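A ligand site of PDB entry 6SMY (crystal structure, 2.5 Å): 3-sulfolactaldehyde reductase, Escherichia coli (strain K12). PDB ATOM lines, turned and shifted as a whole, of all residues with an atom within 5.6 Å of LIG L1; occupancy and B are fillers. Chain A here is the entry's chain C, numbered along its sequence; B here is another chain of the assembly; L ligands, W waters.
An oxygen (O2) of LIG L1 is in hydrogen-bond range of the backbone NH of Gln 11 (2.7 Å). N of Met 12 is in hydrogen-bond range of O8 of LIG L1 (2.8 Å). An oxygen (O12) of LIG L1 sits at hydrogen-bond distance from the backbone carbonyl oxygen of Leu 65, at 2.8 Å. An oxygen (O5) of LIG L1 lies within hydrogen-bond range of the side-chain carboxylate (OD2) of Asp 31 (2.8 Å). NZ of Lys 240 of chain B sits at hydrogen-bond distance from O13 of LIG L1, 2.9 Å away. N of Thr 96 lies within hydrogen-bond range of O12 of LIG L1. O of Thr 96 lies within hydrogen-bond range of O12 of LIG L1, 3.4 Å away. The backbone NH (N) of Gly 10 lies close to an oxygen (O5) of LIG L1 (3.4 Å). The backbone carbonyl oxygen (O) of Ala 232 of chain B is in hydrogen-bond range of a nitrogen (N7) of LIG L1, 3.3 Å away. N of Val 32 lies within hydrogen-bond range of N5 of LIG L1 (3.3 Å). The backbone NH of Ser 125 sits at hydrogen-bond distance from an oxygen (O14) of LIG L1. An oxygen (O1) of LG2 L2 lies within hydrogen-bond range of the backbone NH of Arg 123 (2.9 Å). The backbone carbonyl oxygen of Arg 123 lies within hydrogen-bond range of an oxygen (O4) of LG2 L2 (2.7 Å). The side-chain amino group of Lys 171 lies within salt-bridge range of an oxygen (O1) of LG2 L2 (3.7 Å).
The side-chain hydroxyl (OG) of Ser 95 is in hydrogen-bond range of the backbone NH (N) of Leu 65 (2.7 Å). The backbone NH of Asn 33 is in hydrogen-bond range of the side-chain carboxylate of Asp 31 (2.8 Å). NZ of Lys 240 of chain B sits at hydrogen-bond distance from O of Thr 96 (2.9 Å). O of Pro 66 sits close to NZ of Lys 240 of chain B (3.2 Å). NZ of Lys 240 of chain B lies within salt-bridge range of OD1 of Asp 241 of chain B. OG of Ser 125 sits at hydrogen-bond distance from O of Ala 232 of chain B, 2.4 Å away. The backbone carbonyl oxygen of Val 121 lies within hydrogen-bond range of the side-chain amino group of Lys 171, at 2.8 Å. N of Leu 70 lies within hydrogen-bond range of OD1 of Asn 67 (3.0 Å).
The side-chain sulfur (SD) of Met 64 sits close to an oxygen (O11) of LIG L1, 3.5 Å away. Residues that only touch LIG L1: Thr 124 (3.1 Å), Arg 123 (3.1 Å), Phe 233 of chain B (3.3 Å), Val 121 (3.3 Å), Leu 237 of chain B (3.4 Å), Leu 70 (3.5 Å), Phe 30 (3.6 Å), Leu 9 (3.7 Å), Val 74 (3.7 Å), Lys 171 (3.7 Å), Met 234 of chain B (3.8 Å), Pro 66 (3.8 Å), Gly 13 (3.8 Å), Asp 241 of chain B (3.9 Å) and Ser 95 (3.99 Å). Hydrophobic or aromatic side chains within 4 Å of LIG L1: Met 12, Phe 30, Val 32, Met 64, Leu 65, Pro 66, Leu 70, Val 74, Val 121, Phe 233 of chain B, Met 234 of chain B and Leu 237 of chain B. The nearest printed residue that does not touch LIG L1 is Gly 8 (4.1 Å).
Water W2 lies within hydrogen-bond range of OD2 of Asp 241 of chain B (2.5 Å), O13 of LIG L1 (2.6 Å), OG1 of Thr 96 (2.8 Å) and O5 of LG2 L2 (3.0 Å). Water W3 lies within hydrogen-bond range of O8 of LIG L1 (2.6 Å), N of Gly 13 (2.7 Å), N of Gly 10 (2.8 Å) and O of Met 64 (3.3 Å). Water W1 lies within hydrogen-bond range of the side-chain amide oxygen (OE1) of Gln 11, the backbone NH (N) of Met 234 of chain B and an oxygen (O9) of LIG L1. Water W4 lies within hydrogen-bond range of O of Met 94 (2.7 Å), N of Val 121 (3.0 Å) and OG1 of Thr 96 (3.0 Å).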
ATOM      1  N   ILE A   7       2.584  23.146   4.479  1.00  0.00           N
ATOM      2  CA  ILE A   7       1.816  23.132   3.212  1.00  0.00           C
ATOM      3  C   ILE A   7       0.559  23.976   3.405  1.00  0.00           C
ATOM      4  O   ILE A   7      -0.286  23.610   4.239  1.00  0.00           O
ATOM      5  CB  ILE A   7       1.513  21.691   2.782  1.00  0.00           C
ATOM      6  CG1 ILE A   7       2.786  20.838   2.754  1.00  0.00           C
ATOM      7  CG2 ILE A   7       0.833  21.719   1.431  1.00  0.00           C
ATOM      8  CD1 ILE A   7       2.564  19.382   3.046  1.00  0.00           C
ATOM      9  N   GLY A   8       0.469  25.080   2.647  1.00  0.00           N
ATOM     10  CA  GLY A   8      -0.609  26.078   2.714  1.00  0.00           C
ATOM     11  C   GLY A   8      -0.096  27.382   3.280  1.00  0.00           C
ATOM     12  O   GLY A   8       0.005  27.461   4.507  1.00  0.00           O
ATOM     13  N   LEU A   9       0.223  28.345   2.414  1.00  0.00           N
ATOM     14  CA  LEU A   9       0.859  29.634   2.786  1.00  0.00           C
ATOM     15  C   LEU A   9      -0.137  30.789   2.578  1.00  0.00           C
ATOM     16  O   LEU A   9       0.286  31.853   2.106  1.00  0.00           O
ATOM     17  CB  LEU A   9       2.132  29.768   1.957  1.00  0.00           C
ATOM     18  CG  LEU A   9       3.132  28.631   2.171  1.00  0.00           C
ATOM     19  CD1 LEU A   9       4.394  28.880   1.366  1.00  0.00           C
ATOM     20  N   GLY A  10      -1.408  30.598   2.969  1.00  0.00           N
ATOM     21  CA  GLY A  10      -2.503  31.576   2.775  1.00  0.00           C
ATOM     22  C   GLY A  10      -2.478  32.683   3.825  1.00  0.00           C
ATOM     23  O   GLY A  10      -1.410  32.944   4.364  1.00  0.00           O
ATOM     24  N   GLN A  11      -3.632  33.314   4.076  1.00  0.00           N
ATOM     25  CA  GLN A  11      -3.799  34.440   5.032  1.00  0.00           C
ATOM     26  C   GLN A  11      -3.368  33.986   6.432  1.00  0.00           C
ATOM     27  O   GLN A  11      -2.838  34.842   7.190  1.00  0.00           O
ATOM     28  CB  GLN A  11      -5.259  34.923   5.064  1.00  0.00           C
ATOM     29  CG  GLN A  11      -5.654  35.868   3.940  1.00  0.00           C
ATOM     30  CD  GLN A  11      -6.698  36.848   4.418  1.00  0.00           C
ATOM     31  OE1 GLN A  11      -7.844  36.508   4.679  1.00  0.00           O
ATOM     32  NE2 GLN A  11      -6.308  38.098   4.562  1.00  0.00           N
ATOM     33  N   MET A  12      -3.566  32.693   6.744  1.00  0.00           N
ATOM     34  CA  MET A  12      -3.170  32.061   8.027  1.00  0.00           C
ATOM     35  C   MET A  12      -1.805  31.387   7.895  1.00  0.00           C
ATOM     36  O   MET A  12      -0.892  31.665   8.703  1.00  0.00           O
ATOM     37  CB  MET A  12      -4.205  31.006   8.424  1.00  0.00           C
ATOM     38  CG  MET A  12      -5.575  31.580   8.744  1.00  0.00           C
ATOM     39  SD  MET A  12      -5.536  32.600  10.226  1.00  0.00           S
ATOM     40  CE  MET A  12      -5.383  31.411  11.552  1.00  0.00           C
ATOM     41  N   GLY A  13      -1.667  30.529   6.888  1.00  0.00           N
ATOM     42  CA  GLY A  13      -0.471  29.710   6.673  1.00  0.00           C
ATOM     43  C   GLY A  13       0.794  30.543   6.656  1.00  0.00           C
ATOM     44  O   GLY A  13       1.741  30.197   7.379  1.00  0.00           O
ATOM     45  N   PHE A  30       5.449  24.421   0.830  1.00  0.00           N
ATOM     46  CA  PHE A  30       4.752  24.234  -0.463  1.00  0.00           C
ATOM     47  C   PHE A  30       3.382  24.931  -0.448  1.00  0.00           C
ATOM     48  O   PHE A  30       2.726  24.984   0.604  1.00  0.00           O
ATOM     49  CB  PHE A  30       4.572  22.750  -0.774  1.00  0.00           C
ATOM     50  CG  PHE A  30       3.784  22.557  -2.047  1.00  0.00           C
ATOM     51  CD1 PHE A  30       4.352  22.832  -3.273  1.00  0.00           C
ATOM     52  CD2 PHE A  30       2.456  22.166  -1.997  1.00  0.00           C
ATOM     53  CE1 PHE A  30       3.615  22.685  -4.438  1.00  0.00           C
ATOM     54  CE2 PHE A  30       1.720  22.006  -3.157  1.00  0.00           C
ATOM     55  CZ  PHE A  30       2.301  22.263  -4.373  1.00  0.00           C
ATOM     56  N   ASP A  31       2.994  25.450  -1.611  1.00  0.00           N
ATOM     57  CA  ASP A  31       1.679  26.098  -1.886  1.00  0.00           C
ATOM     58  C   ASP A  31       1.504  26.125  -3.409  1.00  0.00           C
ATOM     59  O   ASP A  31       2.535  26.230  -4.110  1.00  0.00           O
ATOM     60  CB  ASP A  31       1.621  27.519  -1.301  1.00  0.00           C
ATOM     61  CG  ASP A  31       0.232  28.143  -1.313  1.00  0.00           C
ATOM     62  OD1 ASP A  31      -0.402  28.235  -2.394  1.00  0.00           O
ATOM     63  OD2 ASP A  31      -0.196  28.548  -0.243  1.00  0.00           O
ATOM     64  N   VAL A  32       0.273  26.070  -3.918  1.00  0.00           N
ATOM     65  CA  VAL A  32       0.049  26.095  -5.400  1.00  0.00           C
ATOM     66  C   VAL A  32       0.366  27.498  -5.942  1.00  0.00           C
ATOM     67  O   VAL A  32       0.743  27.582  -7.113  1.00  0.00           O
ATOM     68  CB  VAL A  32      -1.338  25.570  -5.835  1.00  0.00           C
ATOM     69  CG1 VAL A  32      -1.424  24.084  -5.552  1.00  0.00           C
ATOM     70  CG2 VAL A  32      -2.502  26.326  -5.205  1.00  0.00           C
ATOM     71  N   ASN A  33       0.336  28.533  -5.104  1.00  0.00           N
ATOM     72  CA  ASN A  33       0.778  29.923  -5.430  1.00  0.00           C
ATOM     73  C   ASN A  33       2.284  30.063  -5.164  1.00  0.00           C
ATOM     74  O   ASN A  33       2.662  30.130  -3.978  1.00  0.00           O
ATOM     75  CB  ASN A  33       0.017  30.990  -4.646  1.00  0.00           C
ATOM     76  CG  ASN A  33       0.502  32.392  -4.948  1.00  0.00           C
ATOM     77  OD1 ASN A  33       0.769  32.728  -6.099  1.00  0.00           O
ATOM     78  ND2 ASN A  33       0.656  33.234  -3.921  1.00  0.00           N
ATOM     79  N   ALA A  36       3.578  32.981  -2.924  1.00  0.00           N
ATOM     80  CA  ALA A  36       3.464  32.695  -1.481  1.00  0.00           C
ATOM     81  C   ALA A  36       4.708  31.904  -1.034  1.00  0.00           C
ATOM     82  O   ALA A  36       5.311  32.265   0.002  1.00  0.00           O
ATOM     83  CB  ALA A  36       2.181  31.943  -1.196  1.00  0.00           C
ATOM     84  N   MET A  64      -2.272  23.763   6.415  1.00  0.00           N
ATOM     85  CA  MET A  64      -3.219  24.870   6.658  1.00  0.00           C
ATOM     86  C   MET A  64      -3.913  25.198   5.336  1.00  0.00           C
ATOM     87  O   MET A  64      -3.438  26.100   4.616  1.00  0.00           O
ATOM     88  CB  MET A  64      -2.484  26.105   7.199  1.00  0.00           C
ATOM     89  CG  MET A  64      -3.417  27.176   7.736  1.00  0.00           C
ATOM     90  SD  MET A  64      -4.571  26.531   9.004  1.00  0.00           S
ATOM     91  CE  MET A  64      -4.749  27.958  10.071  1.00  0.00           C
ATOM     92  N   LEU A  65      -5.002  24.485   5.025  1.00  0.00           N
ATOM     93  CA  LEU A  65      -5.695  24.521   3.719  1.00  0.00           C
ATOM     94  C   LEU A  65      -7.176  24.840   3.915  1.00  0.00           C
ATOM     95  O   LEU A  65      -7.722  24.668   4.994  1.00  0.00           O
ATOM     96  CB  LEU A  65      -5.482  23.180   3.018  1.00  0.00           C
ATOM     97  CG  LEU A  65      -4.032  22.869   2.673  1.00  0.00           C
ATOM     98  CD1 LEU A  65      -3.829  21.377   2.386  1.00  0.00           C
ATOM     99  CD2 LEU A  65      -3.568  23.731   1.505  1.00  0.00           C
ATOM    100  N   PRO A  66      -7.871  25.295   2.841  1.00  0.00           N
ATOM    101  CA  PRO A  66      -9.269  25.719   2.903  1.00  0.00           C
ATOM    102  C   PRO A  66     -10.317  24.638   3.199  1.00  0.00           C
ATOM    103  O   PRO A  66     -11.364  25.014   3.652  1.00  0.00           O
ATOM    104  CB  PRO A  66      -9.556  26.274   1.483  1.00  0.00           C
ATOM    105  CG  PRO A  66      -8.193  26.618   0.942  1.00  0.00           C
ATOM    106  CD  PRO A  66      -7.300  25.534   1.503  1.00  0.00           C
ATOM    107  N   ASN A  67     -10.059  23.368   2.865  1.00  0.00           N
ATOM    108  CA  ASN A  67     -11.047  22.269   3.025  1.00  0.00           C
ATOM    109  C   ASN A  67     -10.353  20.907   3.111  1.00  0.00           C
ATOM    110  O   ASN A  67      -9.167  20.780   2.721  1.00  0.00           O
ATOM    111  CB  ASN A  67     -12.081  22.282   1.898  1.00  0.00           C
ATOM    112  CG  ASN A  67     -11.483  22.045   0.525  1.00  0.00           C
ATOM    113  OD1 ASN A  67     -10.975  20.953   0.248  1.00  0.00           O
ATOM    114  ND2 ASN A  67     -11.541  23.049  -0.339  1.00  0.00           N
ATOM    115  N   LEU A  70      -8.674  19.089  -0.161  1.00  0.00           N
ATOM    116  CA  LEU A  70      -7.320  19.633  -0.465  1.00  0.00           C
ATOM    117  C   LEU A  70      -6.316  19.082   0.562  1.00  0.00           C
ATOM    118  O   LEU A  70      -5.161  18.841   0.176  1.00  0.00           O
ATOM    119  CB  LEU A  70      -7.353  21.175  -0.430  1.00  0.00           C
ATOM    120  CG  LEU A  70      -8.058  21.856  -1.605  1.00  0.00           C
ATOM    121  CD1 LEU A  70      -8.056  23.370  -1.457  1.00  0.00           C
ATOM    122  CD2 LEU A  70      -7.450  21.473  -2.946  1.00  0.00           C
ATOM    123  N   VAL A  74      -3.293  16.585  -0.565  1.00  0.00           N
ATOM    124  CA  VAL A  74      -1.932  17.058  -0.179  1.00  0.00           C
ATOM    125  C   VAL A  74      -1.229  15.965   0.627  1.00  0.00           C
ATOM    126  O   VAL A  74       0.010  15.898   0.573  1.00  0.00           O
ATOM    127  CB  VAL A  74      -1.997  18.405   0.584  1.00  0.00           C
ATOM    128  CG1 VAL A  74      -0.948  18.548   1.662  1.00  0.00           C
ATOM    129  CG2 VAL A  74      -1.941  19.582  -0.383  1.00  0.00           C
ATOM    130  N   MET A  94      -3.979  21.942  10.916  1.00  0.00           N
ATOM    131  CA  MET A  94      -4.473  23.131  11.631  1.00  0.00           C
ATOM    132  C   MET A  94      -5.623  23.767  10.829  1.00  0.00           C
ATOM    133  O   MET A  94      -6.062  24.868  11.212  1.00  0.00           O
ATOM    134  CB  MET A  94      -3.319  24.112  11.855  1.00  0.00           C
ATOM    135  CG  MET A  94      -2.094  23.444  12.484  1.00  0.00           C
ATOM    136  SD  MET A  94      -0.820  24.583  13.028  1.00  0.00           S
ATOM    137  CE  MET A  94      -1.611  25.476  14.363  1.00  0.00           C
ATOM    138  N   SER A  95      -6.114  23.067   9.801  1.00  0.00           N
ATOM    139  CA  SER A  95      -7.196  23.528   8.891  1.00  0.00           C
ATOM    140  C   SER A  95      -8.559  23.475   9.594  1.00  0.00           C
ATOM    141  O   SER A  95      -8.727  22.695  10.544  1.00  0.00           O
ATOM    142  CB  SER A  95      -7.224  22.713   7.618  1.00  0.00           C
ATOM    143  OG  SER A  95      -6.015  22.823   6.897  1.00  0.00           O
ATOM    144  N   THR A  96      -9.496  24.288   9.144  1.00  0.00           N
ATOM    145  CA  THR A  96     -10.927  24.134   9.486  1.00  0.00           C
ATOM    146  C   THR A  96     -11.565  23.260   8.409  1.00  0.00           C
ATOM    147  O   THR A  96     -11.813  23.734   7.299  1.00  0.00           O
ATOM    148  CB  THR A  96     -11.612  25.488   9.649  1.00  0.00           C
ATOM    149  OG1 THR A  96     -10.823  26.251  10.569  1.00  0.00           O
ATOM    150  CG2 THR A  96     -13.039  25.314  10.132  1.00  0.00           C
ATOM    151  N   ILE A  97     -11.791  21.982   8.727  1.00  0.00           N
ATOM    152  CA  ILE A  97     -12.436  21.008   7.806  1.00  0.00           C
ATOM    153  C   ILE A  97     -13.520  20.280   8.598  1.00  0.00           C
ATOM    154  O   ILE A  97     -13.676  20.559   9.819  1.00  0.00           O
ATOM    155  CB  ILE A  97     -11.398  20.065   7.206  1.00  0.00           C
ATOM    156  CG1 ILE A  97     -10.793  19.112   8.234  1.00  0.00           C
ATOM    157  CG2 ILE A  97     -10.314  20.871   6.498  1.00  0.00           C
ATOM    158  CD1 ILE A  97      -9.867  18.058   7.626  1.00  0.00           C
ATOM    159  N   VAL A 121      -7.093  26.531  14.781  1.00  0.00           N
ATOM    160  CA  VAL A 121      -6.806  27.743  15.602  1.00  0.00           C
ATOM    161  C   VAL A 121      -8.048  28.628  15.644  1.00  0.00           C
ATOM    162  O   VAL A 121      -8.749  28.672  14.648  1.00  0.00           O
ATOM    163  CB  VAL A 121      -5.576  28.492  15.068  1.00  0.00           C
ATOM    164  CG1 VAL A 121      -4.300  27.702  15.338  1.00  0.00           C
ATOM    165  CG2 VAL A 121      -5.699  28.789  13.581  1.00  0.00           C
ATOM    166  N   GLY A 122      -8.283  29.277  16.778  1.00  0.00           N
ATOM    167  CA  GLY A 122      -9.258  30.346  16.967  1.00  0.00           C
ATOM    168  C   GLY A 122      -8.595  31.689  16.732  1.00  0.00           C
ATOM    169  O   GLY A 122      -7.349  31.724  16.722  1.00  0.00           O
ATOM    170  N   ARG A 123      -9.403  32.712  16.483  1.00  0.00           N
ATOM    171  CA  ARG A 123      -8.994  34.095  16.108  1.00  0.00           C
ATOM    172  C   ARG A 123      -8.592  34.122  14.631  1.00  0.00           C
ATOM    173  O   ARG A 123      -8.469  33.058  14.013  1.00  0.00           O
ATOM    174  CB  ARG A 123      -7.907  34.624  17.036  1.00  0.00           C
ATOM    175  CG  ARG A 123      -8.384  34.902  18.452  1.00  0.00           C
ATOM    176  CD  ARG A 123      -7.248  35.255  19.407  1.00  0.00           C
ATOM    177  NE  ARG A 123      -7.667  35.050  20.784  1.00  0.00           N
ATOM    178  CZ  ARG A 123      -6.921  34.552  21.760  1.00  0.00           C
ATOM    179  NH1 ARG A 123      -5.641  34.258  21.548  1.00  0.00           N
ATOM    180  NH2 ARG A 123      -7.444  34.406  22.960  1.00  0.00           N
ATOM    181  N   THR A 124      -8.382  35.335  14.112  1.00  0.00           N
ATOM    182  CA  THR A 124      -8.273  35.653  12.674  1.00  0.00           C
ATOM    183  C   THR A 124      -6.804  35.824  12.291  1.00  0.00           C
ATOM    184  O   THR A 124      -5.931  35.579  13.149  1.00  0.00           O
ATOM    185  CB  THR A 124      -9.065  36.917  12.357  1.00  0.00           C
ATOM    186  OG1 THR A 124      -8.325  38.045  12.857  1.00  0.00           O
ATOM    187  CG2 THR A 124     -10.461  36.850  12.913  1.00  0.00           C
ATOM    188  N   SER A 125      -6.573  36.240  11.038  1.00  0.00           N
ATOM    189  CA  SER A 125      -5.240  36.376  10.398  1.00  0.00           C
ATOM    190  C   SER A 125      -4.450  37.529  11.032  1.00  0.00           C
ATOM    191  O   SER A 125      -3.218  37.470  10.960  1.00  0.00           O
ATOM    192  CB  SER A 125      -5.372  36.515   8.899  1.00  0.00           C
ATOM    193  OG  SER A 125      -6.290  37.528   8.548  1.00  0.00           O
ATOM    194  N   LEU A 133      -2.692  33.425  18.082  1.00  0.00           N
ATOM    195  CA  LEU A 133      -3.813  32.491  17.797  1.00  0.00           C
ATOM    196  C   LEU A 133      -4.169  31.716  19.069  1.00  0.00           C
ATOM    197  O   LEU A 133      -3.317  31.549  19.937  1.00  0.00           O
ATOM    198  CB  LEU A 133      -3.429  31.536  16.673  1.00  0.00           C
ATOM    199  CG  LEU A 133      -3.202  32.168  15.313  1.00  0.00           C
ATOM    200  CD1 LEU A 133      -2.645  31.129  14.328  1.00  0.00           C
ATOM    201  CD2 LEU A 133      -4.485  32.803  14.785  1.00  0.00           C
ATOM    202  N   LYS A 171     -13.384  23.739  17.498  1.00  0.00           N
ATOM    203  CA  LYS A 171     -13.244  24.768  16.429  1.00  0.00           C
ATOM    204  C   LYS A 171     -14.590  24.993  15.745  1.00  0.00           C
ATOM    205  O   LYS A 171     -14.939  26.158  15.538  1.00  0.00           O
ATOM    206  CB  LYS A 171     -12.218  24.333  15.382  1.00  0.00           C
ATOM    207  CG  LYS A 171     -12.061  25.295  14.216  1.00  0.00           C
ATOM    208  CD  LYS A 171     -11.752  26.701  14.617  1.00  0.00           C
ATOM    209  CE  LYS A 171     -11.437  27.523  13.394  1.00  0.00           C
ATOM    210  NZ  LYS A 171     -11.408  28.961  13.695  1.00  0.00           N
ATOM    211  N   ALA B 232      -9.527  39.859   7.221  1.00  0.00           N
ATOM    212  CA  ALA B 232      -8.849  39.099   8.299  1.00  0.00           C
ATOM    213  C   ALA B 232      -9.368  37.656   8.232  1.00  0.00           C
ATOM    214  O   ALA B 232      -8.558  36.725   8.289  1.00  0.00           O
ATOM    215  CB  ALA B 232      -9.105  39.744   9.638  1.00  0.00           C
ATOM    216  N   PHE B 233     -10.684  37.513   8.078  1.00  0.00           N
ATOM    217  CA  PHE B 233     -11.390  36.233   7.820  1.00  0.00           C
ATOM    218  C   PHE B 233     -12.384  36.459   6.684  1.00  0.00           C
ATOM    219  O   PHE B 233     -13.344  37.248   6.817  1.00  0.00           O
ATOM    220  CB  PHE B 233     -12.067  35.725   9.097  1.00  0.00           C
ATOM    221  CG  PHE B 233     -12.601  34.326   9.009  1.00  0.00           C
ATOM    222  CD1 PHE B 233     -11.910  33.340   8.349  1.00  0.00           C
ATOM    223  CD2 PHE B 233     -13.814  33.996   9.616  1.00  0.00           C
ATOM    224  CE1 PHE B 233     -12.388  32.048   8.290  1.00  0.00           C
ATOM    225  CE2 PHE B 233     -14.304  32.695   9.558  1.00  0.00           C
ATOM    226  CZ  PHE B 233     -13.587  31.735   8.900  1.00  0.00           C
ATOM    227  N   MET B 234     -12.146  35.757   5.571  1.00  0.00           N
ATOM    228  CA  MET B 234     -12.891  35.918   4.319  1.00  0.00           C
ATOM    229  C   MET B 234     -14.290  35.305   4.457  1.00  0.00           C
ATOM    230  O   MET B 234     -14.445  34.238   5.045  1.00  0.00           O
ATOM    231  CB  MET B 234     -12.134  35.278   3.152  1.00  0.00           C
ATOM    232  CG  MET B 234     -10.971  36.123   2.642  1.00  0.00           C
ATOM    233  SD  MET B 234     -10.228  35.558   1.047  1.00  0.00           S
ATOM    234  CE  MET B 234      -9.414  34.030   1.500  1.00  0.00           C
ATOM    235  N   LEU B 237     -14.737  31.661   3.351  1.00  0.00           N
ATOM    236  CA  LEU B 237     -14.290  30.671   4.352  1.00  0.00           C
ATOM    237  C   LEU B 237     -15.329  30.597   5.481  1.00  0.00           C
ATOM    238  O   LEU B 237     -15.683  29.490   5.871  1.00  0.00           O
ATOM    239  CB  LEU B 237     -12.903  31.079   4.838  1.00  0.00           C
ATOM    240  CG  LEU B 237     -11.764  30.902   3.845  1.00  0.00           C
ATOM    241  CD1 LEU B 237     -10.418  31.256   4.474  1.00  0.00           C
ATOM    242  CD2 LEU B 237     -11.721  29.493   3.295  1.00  0.00           C
ATOM    243  N   LYS B 240     -18.096  28.630   4.177  1.00  0.00           N
ATOM    244  CA  LYS B 240     -17.707  27.187   4.133  1.00  0.00           C
ATOM    245  C   LYS B 240     -17.849  26.585   5.532  1.00  0.00           C
ATOM    246  O   LYS B 240     -18.370  25.461   5.639  1.00  0.00           O
ATOM    247  CB  LYS B 240     -16.299  27.051   3.524  1.00  0.00           C
ATOM    248  CG  LYS B 240     -15.623  25.689   3.594  1.00  0.00           C
ATOM    249  CD  LYS B 240     -14.723  25.431   4.822  1.00  0.00           C
ATOM    250  CE  LYS B 240     -13.670  26.504   5.046  1.00  0.00           C
ATOM    251  NZ  LYS B 240     -12.824  26.283   6.242  1.00  0.00           N
ATOM    252  N   ASP B 241     -17.375  27.260   6.579  1.00  0.00           N
ATOM    253  CA  ASP B 241     -17.399  26.749   7.976  1.00  0.00           C
ATOM    254  C   ASP B 241     -18.862  26.535   8.383  1.00  0.00           C
ATOM    255  O   ASP B 241     -19.147  25.517   8.988  1.00  0.00           O
ATOM    256  CB  ASP B 241     -16.678  27.682   8.954  1.00  0.00           C
ATOM    257  CG  ASP B 241     -15.158  27.609   8.869  1.00  0.00           C
ATOM    258  OD1 ASP B 241     -14.646  26.850   8.046  1.00  0.00           O
ATOM    259  OD2 ASP B 241     -14.519  28.349   9.625  1.00  0.00           O
HETATM  260  P1  LIG L   1      -6.316  31.301   2.367  1.00  0.00           P
HETATM  261  O1  LIG L   1      -7.158  31.031   1.162  1.00  0.00           O
HETATM  262  O2  LIG L   1      -5.703  32.658   2.545  1.00  0.00           O
HETATM  263  O3  LIG L   1      -5.180  30.176   2.487  1.00  0.00           O
HETATM  264  C1  LIG L   1      -5.214  28.988   1.661  1.00  0.00           C
HETATM  265  C2  LIG L   1      -3.891  28.854   0.957  1.00  0.00           C
HETATM  266  O4  LIG L   1      -3.740  27.482   0.500  1.00  0.00           O
HETATM  267  C3  LIG L   1      -3.677  29.743  -0.288  1.00  0.00           C
HETATM  268  O5  LIG L   1      -2.378  30.325  -0.272  1.00  0.00           O
HETATM  269  C4  LIG L   1      -3.826  28.764  -1.452  1.00  0.00           C
HETATM  270  O6  LIG L   1      -3.081  29.213  -2.559  1.00  0.00           O
HETATM  271  C5  LIG L   1      -3.260  27.485  -0.820  1.00  0.00           C
HETATM  272  N1  LIG L   1      -3.651  26.215  -1.441  1.00  0.00           N
HETATM  273  C6  LIG L   1      -4.903  25.819  -1.844  1.00  0.00           C
HETATM  274  N2  LIG L   1      -4.936  24.604  -2.332  1.00  0.00           N
HETATM  275  C7  LIG L   1      -3.632  24.143  -2.199  1.00  0.00           C
HETATM  276  C8  LIG L   1      -3.008  22.911  -2.504  1.00  0.00           C
HETATM  277  N3  LIG L   1      -3.636  21.857  -3.013  1.00  0.00           N
HETATM  278  N4  LIG L   1      -1.681  22.794  -2.218  1.00  0.00           N
HETATM  279  C9  LIG L   1      -1.046  23.840  -1.692  1.00  0.00           C
HETATM  280  N5  LIG L   1      -1.524  25.051  -1.371  1.00  0.00           N
HETATM  281  C10 LIG L   1      -2.836  25.137  -1.642  1.00  0.00           C
HETATM  282  O7  LIG L   1      -7.138  30.989   3.721  1.00  0.00           O
HETATM  283  P2  LIG L   1      -6.656  31.106   5.264  1.00  0.00           P
HETATM  284  O8  LIG L   1      -5.169  30.898   5.386  1.00  0.00           O
HETATM  285  O9  LIG L   1      -7.188  32.384   5.824  1.00  0.00           O
HETATM  286  O10 LIG L   1      -7.406  29.868   5.956  1.00  0.00           O
HETATM  287  C11 LIG L   1      -6.746  28.563   6.001  1.00  0.00           C
HETATM  288  C12 LIG L   1      -7.567  27.592   6.823  1.00  0.00           C
HETATM  289  O11 LIG L   1      -7.595  28.020   8.205  1.00  0.00           O
HETATM  290  C13 LIG L   1      -9.038  27.417   6.421  1.00  0.00           C
HETATM  291  O12 LIG L   1      -9.435  26.084   6.710  1.00  0.00           O
HETATM  292  C14 LIG L   1      -9.709  28.485   7.288  1.00  0.00           C
HETATM  293  O13 LIG L   1     -11.119  28.295   7.358  1.00  0.00           O
HETATM  294  C15 LIG L   1      -8.942  28.274   8.601  1.00  0.00           C
HETATM  295  N6  LIG L   1      -8.894  29.439   9.539  1.00  0.00           N
HETATM  296  C16 LIG L   1      -8.952  30.748   9.064  1.00  0.00           C
HETATM  297  C17 LIG L   1      -8.718  31.818   9.921  1.00  0.00           C
HETATM  298  C18 LIG L   1      -8.792  33.230   9.360  1.00  0.00           C
HETATM  299  O14 LIG L   1      -9.063  34.170  10.118  1.00  0.00           O
HETATM  300  N7  LIG L   1      -8.585  33.395   8.058  1.00  0.00           N
HETATM  301  C19 LIG L   1      -8.416  31.552  11.260  1.00  0.00           C
HETATM  302  C20 LIG L   1      -8.496  30.252  11.745  1.00  0.00           C
HETATM  303  C21 LIG L   1      -8.725  29.211  10.865  1.00  0.00           C
HETATM  304  C1  LG2 L   2     -12.877  33.062  13.709  1.00  0.00           C
HETATM  305  O1  LG2 L   2     -12.146  31.845  15.898  1.00  0.00           O
HETATM  306  C2  LG2 L   2     -11.506  32.727  13.161  1.00  0.00           C
HETATM  307  O2  LG2 L   2     -12.586  34.297  15.979  1.00  0.00           O
HETATM  308  C3  LG2 L   2     -11.612  32.111  11.788  1.00  0.00           C
HETATM  309  O3  LG2 L   2     -14.463  32.756  15.725  1.00  0.00           O
HETATM  310  S1  LG2 L   2     -13.072  33.047  15.486  1.00  0.00           S
HETATM  311  O4  LG2 L   2     -10.823  31.822  14.005  1.00  0.00           O
HETATM  312  O5  LG2 L   2     -11.657  30.685  11.850  1.00  0.00           O
HETATM  313  O   HOH W   1      -9.378  34.486   5.248  1.00  0.00           O
HETATM  314  O   HOH W   2     -12.001  28.648   9.739  1.00  0.00           O
HETATM  315  O   HOH W   3      -3.133  29.397   4.888  1.00  0.00           O
HETATM  316  O   HOH W   4      -8.266  26.180  12.097  1.00  0.00           O
